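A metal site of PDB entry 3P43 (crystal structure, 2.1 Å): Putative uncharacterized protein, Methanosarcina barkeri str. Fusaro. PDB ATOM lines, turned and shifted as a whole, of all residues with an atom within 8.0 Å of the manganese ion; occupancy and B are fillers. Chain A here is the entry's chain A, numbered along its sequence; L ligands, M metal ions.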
ATOM      1  N   GLN A  35     -30.033   1.746  10.541  1.00  0.00           N
ATOM      2  CA  GLN A  35     -29.667   0.383  10.199  1.00  0.00           C
ATOM      3  C   GLN A  35     -28.154   0.200  10.243  1.00  0.00           C
ATOM      4  O   GLN A  35     -27.404   0.917   9.566  1.00  0.00           O
ATOM      5  CB  GLN A  35     -30.214   0.005   8.813  1.00  0.00           C
ATOM      6  CG  GLN A  35     -31.674  -0.461   8.829  1.00  0.00           C
ATOM      7  CD  GLN A  35     -32.371  -0.262   7.496  1.00  0.00           C
ATOM      8  OE1 GLN A  35     -32.026   0.641   6.745  1.00  0.00           O
ATOM      9  NE2 GLN A  35     -33.363  -1.097   7.209  1.00  0.00           N
ATOM     10  N   ARG A  36     -27.702  -0.749  11.053  1.00  0.00           N
ATOM     11  CA  ARG A  36     -26.319  -1.174  11.029  1.00  0.00           C
ATOM     12  C   ARG A  36     -26.128  -1.963   9.743  1.00  0.00           C
ATOM     13  O   ARG A  36     -26.807  -2.960   9.510  1.00  0.00           O
ATOM     14  CB  ARG A  36     -26.000  -2.066  12.221  1.00  0.00           C
ATOM     15  CG  ARG A  36     -24.513  -2.333  12.394  1.00  0.00           C
ATOM     16  CD  ARG A  36     -24.252  -3.243  13.566  1.00  0.00           C
ATOM     17  NE  ARG A  36     -24.615  -4.631  13.280  1.00  0.00           N
ATOM     18  CZ  ARG A  36     -25.086  -5.487  14.175  1.00  0.00           C
ATOM     19  NH1 ARG A  36     -25.260  -5.096  15.433  1.00  0.00           N
ATOM     20  NH2 ARG A  36     -25.388  -6.727  13.832  1.00  0.00           N
ATOM     21  N   HIS A  37     -25.191  -1.511   8.906  1.00  0.00           N
ATOM     22  CA  HIS A  37     -24.990  -2.136   7.612  1.00  0.00           C
ATOM     23  C   HIS A  37     -23.603  -2.762   7.548  1.00  0.00           C
ATOM     24  O   HIS A  37     -22.595  -2.060   7.554  1.00  0.00           O
ATOM     25  CB  HIS A  37     -25.160  -1.100   6.495  1.00  0.00           C
ATOM     26  CG  HIS A  37     -25.196  -1.689   5.120  1.00  0.00           C
ATOM     27  ND1 HIS A  37     -25.178  -0.921   3.982  1.00  0.00           N
ATOM     28  CD2 HIS A  37     -25.266  -2.981   4.707  1.00  0.00           C
ATOM     29  CE1 HIS A  37     -25.219  -1.703   2.920  1.00  0.00           C
ATOM     30  NE2 HIS A  37     -25.273  -2.958   3.335  1.00  0.00           N
ATOM     31  N   ASP A  38     -23.551  -4.083   7.509  1.00  0.00           N
ATOM     32  CA  ASP A  38     -22.292  -4.815   7.402  1.00  0.00           C
ATOM     33  C   ASP A  38     -21.965  -5.049   5.920  1.00  0.00           C
ATOM     34  O   ASP A  38     -22.376  -6.056   5.344  1.00  0.00           O
ATOM     35  CB  ASP A  38     -22.384  -6.157   8.137  1.00  0.00           C
ATOM     36  CG  ASP A  38     -21.018  -6.772   8.419  1.00  0.00           C
ATOM     37  OD1 ASP A  38     -20.002  -6.199   7.965  1.00  0.00           O
ATOM     38  OD2 ASP A  38     -20.957  -7.809   9.103  1.00  0.00           O
ATOM     39  N   ALA A  39     -21.226  -4.130   5.325  1.00  0.00           N
ATOM     40  CA  ALA A  39     -20.922  -4.217   3.899  1.00  0.00           C
ATOM     41  C   ALA A  39     -19.412  -4.330   3.703  1.00  0.00           C
ATOM     42  O   ALA A  39     -18.774  -5.186   4.324  1.00  0.00           O
ATOM     43  CB  ALA A  39     -21.459  -2.989   3.167  1.00  0.00           C
ATOM     44  N   LYS A  41     -17.321  -2.137   4.750  1.00  0.00           N
ATOM     45  CA  LYS A  41     -16.991  -1.900   6.137  1.00  0.00           C
ATOM     46  C   LYS A  41     -18.284  -1.894   6.917  1.00  0.00           C
ATOM     47  O   LYS A  41     -19.369  -1.745   6.337  1.00  0.00           O
ATOM     48  CB  LYS A  41     -16.309  -0.543   6.308  1.00  0.00           C
ATOM     49  CG  LYS A  41     -15.576  -0.077   5.063  1.00  0.00           C
ATOM     50  CD  LYS A  41     -14.080  -0.245   5.223  1.00  0.00           C
ATOM     51  CE  LYS A  41     -13.533   0.664   6.312  1.00  0.00           C
ATOM     52  NZ  LYS A  41     -12.041   0.686   6.315  1.00  0.00           N
ATOM     53  N   LEU A  42     -18.184  -2.061   8.227  1.00  0.00           N
ATOM     54  CA  LEU A  42     -19.336  -1.931   9.103  1.00  0.00           C
ATOM     55  C   LEU A  42     -19.616  -0.437   9.286  1.00  0.00           C
ATOM     56  O   LEU A  42     -18.723   0.320   9.672  1.00  0.00           O
ATOM     57  CB  LEU A  42     -19.044  -2.584  10.457  1.00  0.00           C
ATOM     58  CG  LEU A  42     -20.185  -2.832  11.449  1.00  0.00           C
ATOM     59  CD1 LEU A  42     -20.791  -1.525  11.969  1.00  0.00           C
ATOM     60  CD2 LEU A  42     -21.253  -3.732  10.822  1.00  0.00           C
ATOM     61  N   HIS A  43     -20.852  -0.024   9.014  1.00  0.00           N
ATOM     62  CA  HIS A  43     -21.255   1.362   9.228  1.00  0.00           C
ATOM     63  C   HIS A  43     -22.728   1.437   9.575  1.00  0.00           C
ATOM     64  O   HIS A  43     -23.409   0.412   9.633  1.00  0.00           O
ATOM     65  CB  HIS A  43     -20.962   2.213   7.988  1.00  0.00           C
ATOM     66  CG  HIS A  43     -21.740   1.799   6.784  1.00  0.00           C
ATOM     67  ND1 HIS A  43     -21.330   0.784   5.943  1.00  0.00           N
ATOM     68  CD2 HIS A  43     -22.914   2.249   6.279  1.00  0.00           C
ATOM     69  CE1 HIS A  43     -22.212   0.641   4.970  1.00  0.00           C
ATOM     70  NE2 HIS A  43     -23.181   1.515   5.152  1.00  0.00           N
ATOM     71  N   TYR A  44     -23.225   2.638   9.807  1.00  0.00           N
ATOM     72  CA  TYR A  44     -24.614   2.812  10.183  1.00  0.00           C
ATOM     73  C   TYR A  44     -25.303   3.734   9.204  1.00  0.00           C
ATOM     74  O   TYR A  44     -24.831   4.829   8.904  1.00  0.00           O
ATOM     75  CB  TYR A  44     -24.737   3.342  11.610  1.00  0.00           C
ATOM     76  CG  TYR A  44     -24.337   2.310  12.651  1.00  0.00           C
ATOM     77  CD1 TYR A  44     -25.302   1.622  13.376  1.00  0.00           C
ATOM     78  CD2 TYR A  44     -23.000   2.024  12.902  1.00  0.00           C
ATOM     79  CE1 TYR A  44     -24.954   0.681  14.321  1.00  0.00           C
ATOM     80  CE2 TYR A  44     -22.628   1.086  13.851  1.00  0.00           C
ATOM     81  CZ  TYR A  44     -23.614   0.415  14.561  1.00  0.00           C
ATOM     82  OH  TYR A  44     -23.267  -0.526  15.507  1.00  0.00           O
ATOM     83  N   ASP A  45     -26.444   3.282   8.685  1.00  0.00           N
ATOM     84  CA  ASP A  45     -27.233   4.112   7.804  1.00  0.00           C
ATOM     85  C   ASP A  45     -28.312   4.805   8.620  1.00  0.00           C
ATOM     86  O   ASP A  45     -29.113   4.161   9.308  1.00  0.00           O
ATOM     87  CB  ASP A  45     -27.823   3.283   6.672  1.00  0.00           C
ATOM     88  CG  ASP A  45     -26.764   2.797   5.702  1.00  0.00           C
ATOM     89  OD1 ASP A  45     -26.034   3.645   5.154  1.00  0.00           O
ATOM     90  OD2 ASP A  45     -26.656   1.577   5.502  1.00  0.00           O
ATOM     91  N   PHE A  46     -28.281   6.135   8.591  1.00  0.00           N
ATOM     92  CA  PHE A  46     -29.234   6.967   9.295  1.00  0.00           C
ATOM     93  C   PHE A  46     -30.240   7.528   8.288  1.00  0.00           C
ATOM     94  O   PHE A  46     -29.852   8.177   7.315  1.00  0.00           O
ATOM     95  CB  PHE A  46     -28.505   8.103  10.020  1.00  0.00           C
ATOM     96  CG  PHE A  46     -29.414   9.064  10.704  1.00  0.00           C
ATOM     97  CD1 PHE A  46     -30.030   8.721  11.903  1.00  0.00           C
ATOM     98  CD2 PHE A  46     -29.688  10.300  10.148  1.00  0.00           C
ATOM     99  CE1 PHE A  46     -30.877   9.594  12.526  1.00  0.00           C
ATOM    100  CE2 PHE A  46     -30.538  11.187  10.779  1.00  0.00           C
ATOM    101  CZ  PHE A  46     -31.139  10.835  11.965  1.00  0.00           C
ATOM    102  N   ARG A  47     -31.524   7.264   8.504  1.00  0.00           N
ATOM    103  CA  ARG A  47     -32.554   7.628   7.533  1.00  0.00           C
ATOM    104  C   ARG A  47     -33.700   8.408   8.153  1.00  0.00           C
ATOM    105  O   ARG A  47     -34.214   8.044   9.216  1.00  0.00           O
ATOM    106  CB  ARG A  47     -33.122   6.369   6.876  1.00  0.00           C
ATOM    107  CG  ARG A  47     -32.097   5.392   6.342  1.00  0.00           C
ATOM    108  CD  ARG A  47     -32.785   4.271   5.593  1.00  0.00           C
ATOM    109  NE  ARG A  47     -31.930   3.106   5.472  1.00  0.00           N
ATOM    110  CZ  ARG A  47     -30.953   2.992   4.587  1.00  0.00           C
ATOM    111  NH1 ARG A  47     -30.707   3.980   3.736  1.00  0.00           N
ATOM    112  NH2 ARG A  47     -30.221   1.890   4.552  1.00  0.00           N
ATOM    113  N   SER A  56     -31.204   9.622   3.318  1.00  0.00           N
ATOM    114  CA  SER A  56     -30.267   8.707   3.966  1.00  0.00           C
ATOM    115  C   SER A  56     -28.825   9.189   4.043  1.00  0.00           C
ATOM    116  O   SER A  56     -28.336   9.877   3.137  1.00  0.00           O
ATOM    117  CB  SER A  56     -30.315   7.345   3.270  1.00  0.00           C
ATOM    118  OG  SER A  56     -31.593   6.752   3.401  1.00  0.00           O
ATOM    119  N   TRP A  57     -28.153   8.806   5.121  1.00  0.00           N
ATOM    120  CA  TRP A  57     -26.733   9.094   5.328  1.00  0.00           C
ATOM    121  C   TRP A  57     -26.010   7.861   5.843  1.00  0.00           C
ATOM    122  O   TRP A  57     -26.546   7.139   6.678  1.00  0.00           O
ATOM    123  CB  TRP A  57     -26.537  10.216   6.360  1.00  0.00           C
ATOM    124  CG  TRP A  57     -27.022  11.586   5.949  1.00  0.00           C
ATOM    125  CD1 TRP A  57     -26.263  12.607   5.451  1.00  0.00           C
ATOM    126  CD2 TRP A  57     -28.363  12.089   6.038  1.00  0.00           C
ATOM    127  NE1 TRP A  57     -27.054  13.710   5.220  1.00  0.00           N
ATOM    128  CE2 TRP A  57     -28.342  13.415   5.575  1.00  0.00           C
ATOM    129  CE3 TRP A  57     -29.575  11.542   6.481  1.00  0.00           C
ATOM    130  CZ2 TRP A  57     -29.494  14.204   5.519  1.00  0.00           C
ATOM    131  CZ3 TRP A  57     -30.710  12.328   6.423  1.00  0.00           C
ATOM    132  CH2 TRP A  57     -30.663  13.643   5.954  1.00  0.00           C
ATOM    133  N   ALA A  58     -24.808   7.628   5.329  1.00  0.00           N
ATOM    134  CA  ALA A  58     -23.914   6.615   5.890  1.00  0.00           C
ATOM    135  C   ALA A  58     -23.022   7.242   6.969  1.00  0.00           C
ATOM    136  O   ALA A  58     -22.315   8.209   6.711  1.00  0.00           O
ATOM    137  CB  ALA A  58     -23.064   6.003   4.797  1.00  0.00           C
ATOM    138  N   VAL A  59     -23.089   6.697   8.177  1.00  0.00           N
ATOM    139  CA  VAL A  59     -22.266   7.148   9.289  1.00  0.00           C
ATOM    140  C   VAL A  59     -21.305   6.027   9.677  1.00  0.00           C
ATOM    141  O   VAL A  59     -21.745   4.952  10.098  1.00  0.00           O
ATOM    142  CB  VAL A  59     -23.142   7.503  10.514  1.00  0.00           C
ATOM    143  CG1 VAL A  59     -22.325   8.215  11.578  1.00  0.00           C
ATOM    144  CG2 VAL A  59     -24.322   8.362  10.077  1.00  0.00           C
ATOM    145  N   THR A  76     -26.384   9.476   1.078  1.00  0.00           N
ATOM    146  CA  THR A  76     -26.487   8.387   0.109  1.00  0.00           C
ATOM    147  C   THR A  76     -27.804   8.573  -0.643  1.00  0.00           C
ATOM    148  O   THR A  76     -28.492   9.585  -0.472  1.00  0.00           O
ATOM    149  CB  THR A  76     -26.477   7.014   0.802  1.00  0.00           C
ATOM    150  OG1 THR A  76     -27.578   6.934   1.723  1.00  0.00           O
ATOM    151  CG2 THR A  76     -25.164   6.800   1.554  1.00  0.00           C
ATOM    152  N   HIS A  79     -34.016   5.916  -0.063  1.00  0.00           N
ATOM    153  CA  HIS A  79     -34.527   4.561  -0.031  1.00  0.00           C
ATOM    154  C   HIS A  79     -36.032   4.639   0.077  1.00  0.00           C
ATOM    155  O   HIS A  79     -36.553   5.616   0.602  1.00  0.00           O
ATOM    156  CB  HIS A  79     -33.965   3.807   1.174  1.00  0.00           C
ATOM    157  CG  HIS A  79     -32.534   3.398   1.003  1.00  0.00           C
ATOM    158  ND1 HIS A  79     -31.524   4.305   0.762  1.00  0.00           N
ATOM    159  CD2 HIS A  79     -31.946   2.176   1.033  1.00  0.00           C
ATOM    160  CE1 HIS A  79     -30.374   3.657   0.656  1.00  0.00           C
ATOM    161  NE2 HIS A  79     -30.604   2.365   0.821  1.00  0.00           N
ATOM    162  N   TYR A  83     -38.238   0.291   3.439  1.00  0.00           N
ATOM    163  CA  TYR A  83     -36.917  -0.160   3.821  1.00  0.00           C
ATOM    164  C   TYR A  83     -36.679   0.033   5.321  1.00  0.00           C
ATOM    165  O   TYR A  83     -35.800  -0.598   5.901  1.00  0.00           O
ATOM    166  CB  TYR A  83     -35.847   0.569   3.016  1.00  0.00           C
ATOM    167  CG  TYR A  83     -34.570  -0.222   2.832  1.00  0.00           C
ATOM    168  CD1 TYR A  83     -34.546  -1.343   2.019  1.00  0.00           C
ATOM    169  CD2 TYR A  83     -33.397   0.151   3.468  1.00  0.00           C
ATOM    170  CE1 TYR A  83     -33.388  -2.078   1.843  1.00  0.00           C
ATOM    171  CE2 TYR A  83     -32.241  -0.569   3.301  1.00  0.00           C
ATOM    172  CZ  TYR A  83     -32.234  -1.688   2.490  1.00  0.00           C
ATOM    173  OH  TYR A  83     -31.074  -2.408   2.314  1.00  0.00           O
ATOM    174  N   TYR A  95     -26.913  -2.592  -5.037  1.00  0.00           N
ATOM    175  CA  TYR A  95     -26.718  -1.394  -4.232  1.00  0.00           C
ATOM    176  C   TYR A  95     -27.228  -1.701  -2.835  1.00  0.00           C
ATOM    177  O   TYR A  95     -28.373  -2.124  -2.664  1.00  0.00           O
ATOM    178  CB  TYR A  95     -27.479  -0.209  -4.811  1.00  0.00           C
ATOM    179  CG  TYR A  95     -27.174   1.109  -4.113  1.00  0.00           C
ATOM    180  CD1 TYR A  95     -26.089   1.884  -4.508  1.00  0.00           C
ATOM    181  CD2 TYR A  95     -27.948   1.565  -3.057  1.00  0.00           C
ATOM    182  CE1 TYR A  95     -25.787   3.082  -3.884  1.00  0.00           C
ATOM    183  CE2 TYR A  95     -27.668   2.766  -2.422  1.00  0.00           C
ATOM    184  CZ  TYR A  95     -26.583   3.520  -2.839  1.00  0.00           C
ATOM    185  OH  TYR A  95     -26.281   4.718  -2.215  1.00  0.00           O
ATOM    186  N   GLY A  96     -26.373  -1.525  -1.835  1.00  0.00           N
ATOM    187  CA  GLY A  96     -26.763  -1.810  -0.463  1.00  0.00           C
ATOM    188  C   GLY A  96     -26.441  -3.230  -0.061  1.00  0.00           C
ATOM    189  O   GLY A  96     -26.877  -3.687   0.996  1.00  0.00           O
ATOM    190  N   ALA A  97     -25.690  -3.938  -0.891  1.00  0.00           N
ATOM    191  CA  ALA A  97     -25.276  -5.323  -0.590  1.00  0.00           C
ATOM    192  C   ALA A  97     -24.694  -5.410   0.818  1.00  0.00           C
ATOM    193  O   ALA A  97     -23.957  -4.527   1.255  1.00  0.00           O
ATOM    194  CB  ALA A  97     -24.265  -5.820  -1.610  1.00  0.00           C
ATOM    195  N   LYS A  99     -25.193  -7.216   5.129  1.00  0.00           N
ATOM    196  CA  LYS A  99     -26.112  -7.554   6.210  1.00  0.00           C
ATOM    197  C   LYS A  99     -26.720  -6.299   6.814  1.00  0.00           C
ATOM    198  O   LYS A  99     -26.010  -5.344   7.137  1.00  0.00           O
ATOM    199  CB  LYS A  99     -25.364  -8.352   7.283  1.00  0.00           C
ATOM    200  CG  LYS A  99     -24.717  -9.622   6.762  1.00  0.00           C
ATOM    201  CD  LYS A  99     -23.701 -10.177   7.740  1.00  0.00           C
ATOM    202  CE  LYS A  99     -23.105 -11.490   7.250  1.00  0.00           C
ATOM    203  NZ  LYS A  99     -24.191 -12.481   6.989  1.00  0.00           N
ATOM    204  N   VAL A 100     -28.035  -6.312   6.993  1.00  0.00           N
ATOM    205  CA  VAL A 100     -28.748  -5.145   7.508  1.00  0.00           C
ATOM    206  C   VAL A 100     -29.522  -5.490   8.778  1.00  0.00           C
ATOM    207  O   VAL A 100     -30.288  -6.442   8.804  1.00  0.00           O
ATOM    208  CB  VAL A 100     -29.736  -4.600   6.466  1.00  0.00           C
ATOM    209  CG1 VAL A 100     -30.522  -3.414   7.041  1.00  0.00           C
ATOM    210  CG2 VAL A 100     -29.012  -4.203   5.186  1.00  0.00           C
HETATM  211  P1  LIG L   1     -24.701   2.349   1.234  1.00  0.00           P
HETATM  212  O1  LIG L   1     -26.030   1.664   1.365  1.00  0.00           O
HETATM  213  O2  LIG L   1     -23.590   1.382   1.570  1.00  0.00           O
HETATM  214  O3  LIG L   1     -24.640   3.517   2.184  1.00  0.00           O
HETATM  215  O4  LIG L   1     -24.526   2.844  -0.186  1.00  0.00           O
HETATM  216 MN    MN M   1     -25.073   1.481   3.923  1.00  0.00          MN
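The side-chain carboxylate (OD2) of Asp 45 sits close to the guanidinium group (NH2) of Arg 47, at 3.7 Å.
O of Lys 41 is in hydrogen-bond range of ND1 of His 43, 3.2 Å away.
The backbone NH (N) of Asp 45 sits at hydrogen-bond distance from the backbone carbonyl oxygen (O) of Gln 35.
NE2 of His 37 lies within hydrogen-bond range of O of Gly 96 (2.9 Å).
NE2 of His 37 lies within hydrogen-bond range of O of Ala 97, 2.9 Å away.
Of the 24 residues printed, 3 come within 4 Å of the manganese ion.
The nearest printed residue that does not touch the manganese ion is Ala 58 (5.0 Å).
The manganese ion is bound by the side-chain carboxylate (OD2) of Asp 45 (2.2 Å), a ring nitrogen (NE2) of His 43 (2.3 Å), a ring nitrogen (ND1) of His 37 (2.4 Å) and the side-chain carboxylate (OD1) of Asp 45 (2.7 Å).
The manganese ion has four donor atoms within binding distance.
Slightly farther from the manganese ion lies an oxygen (O3) of the ligand (2.7 Å).
Slightly farther from the manganese ion lies O1 of the ligand (2.7 Å).
Slightly farther from the manganese ion lies an oxygen (O2) of the ligand (2.8 Å).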
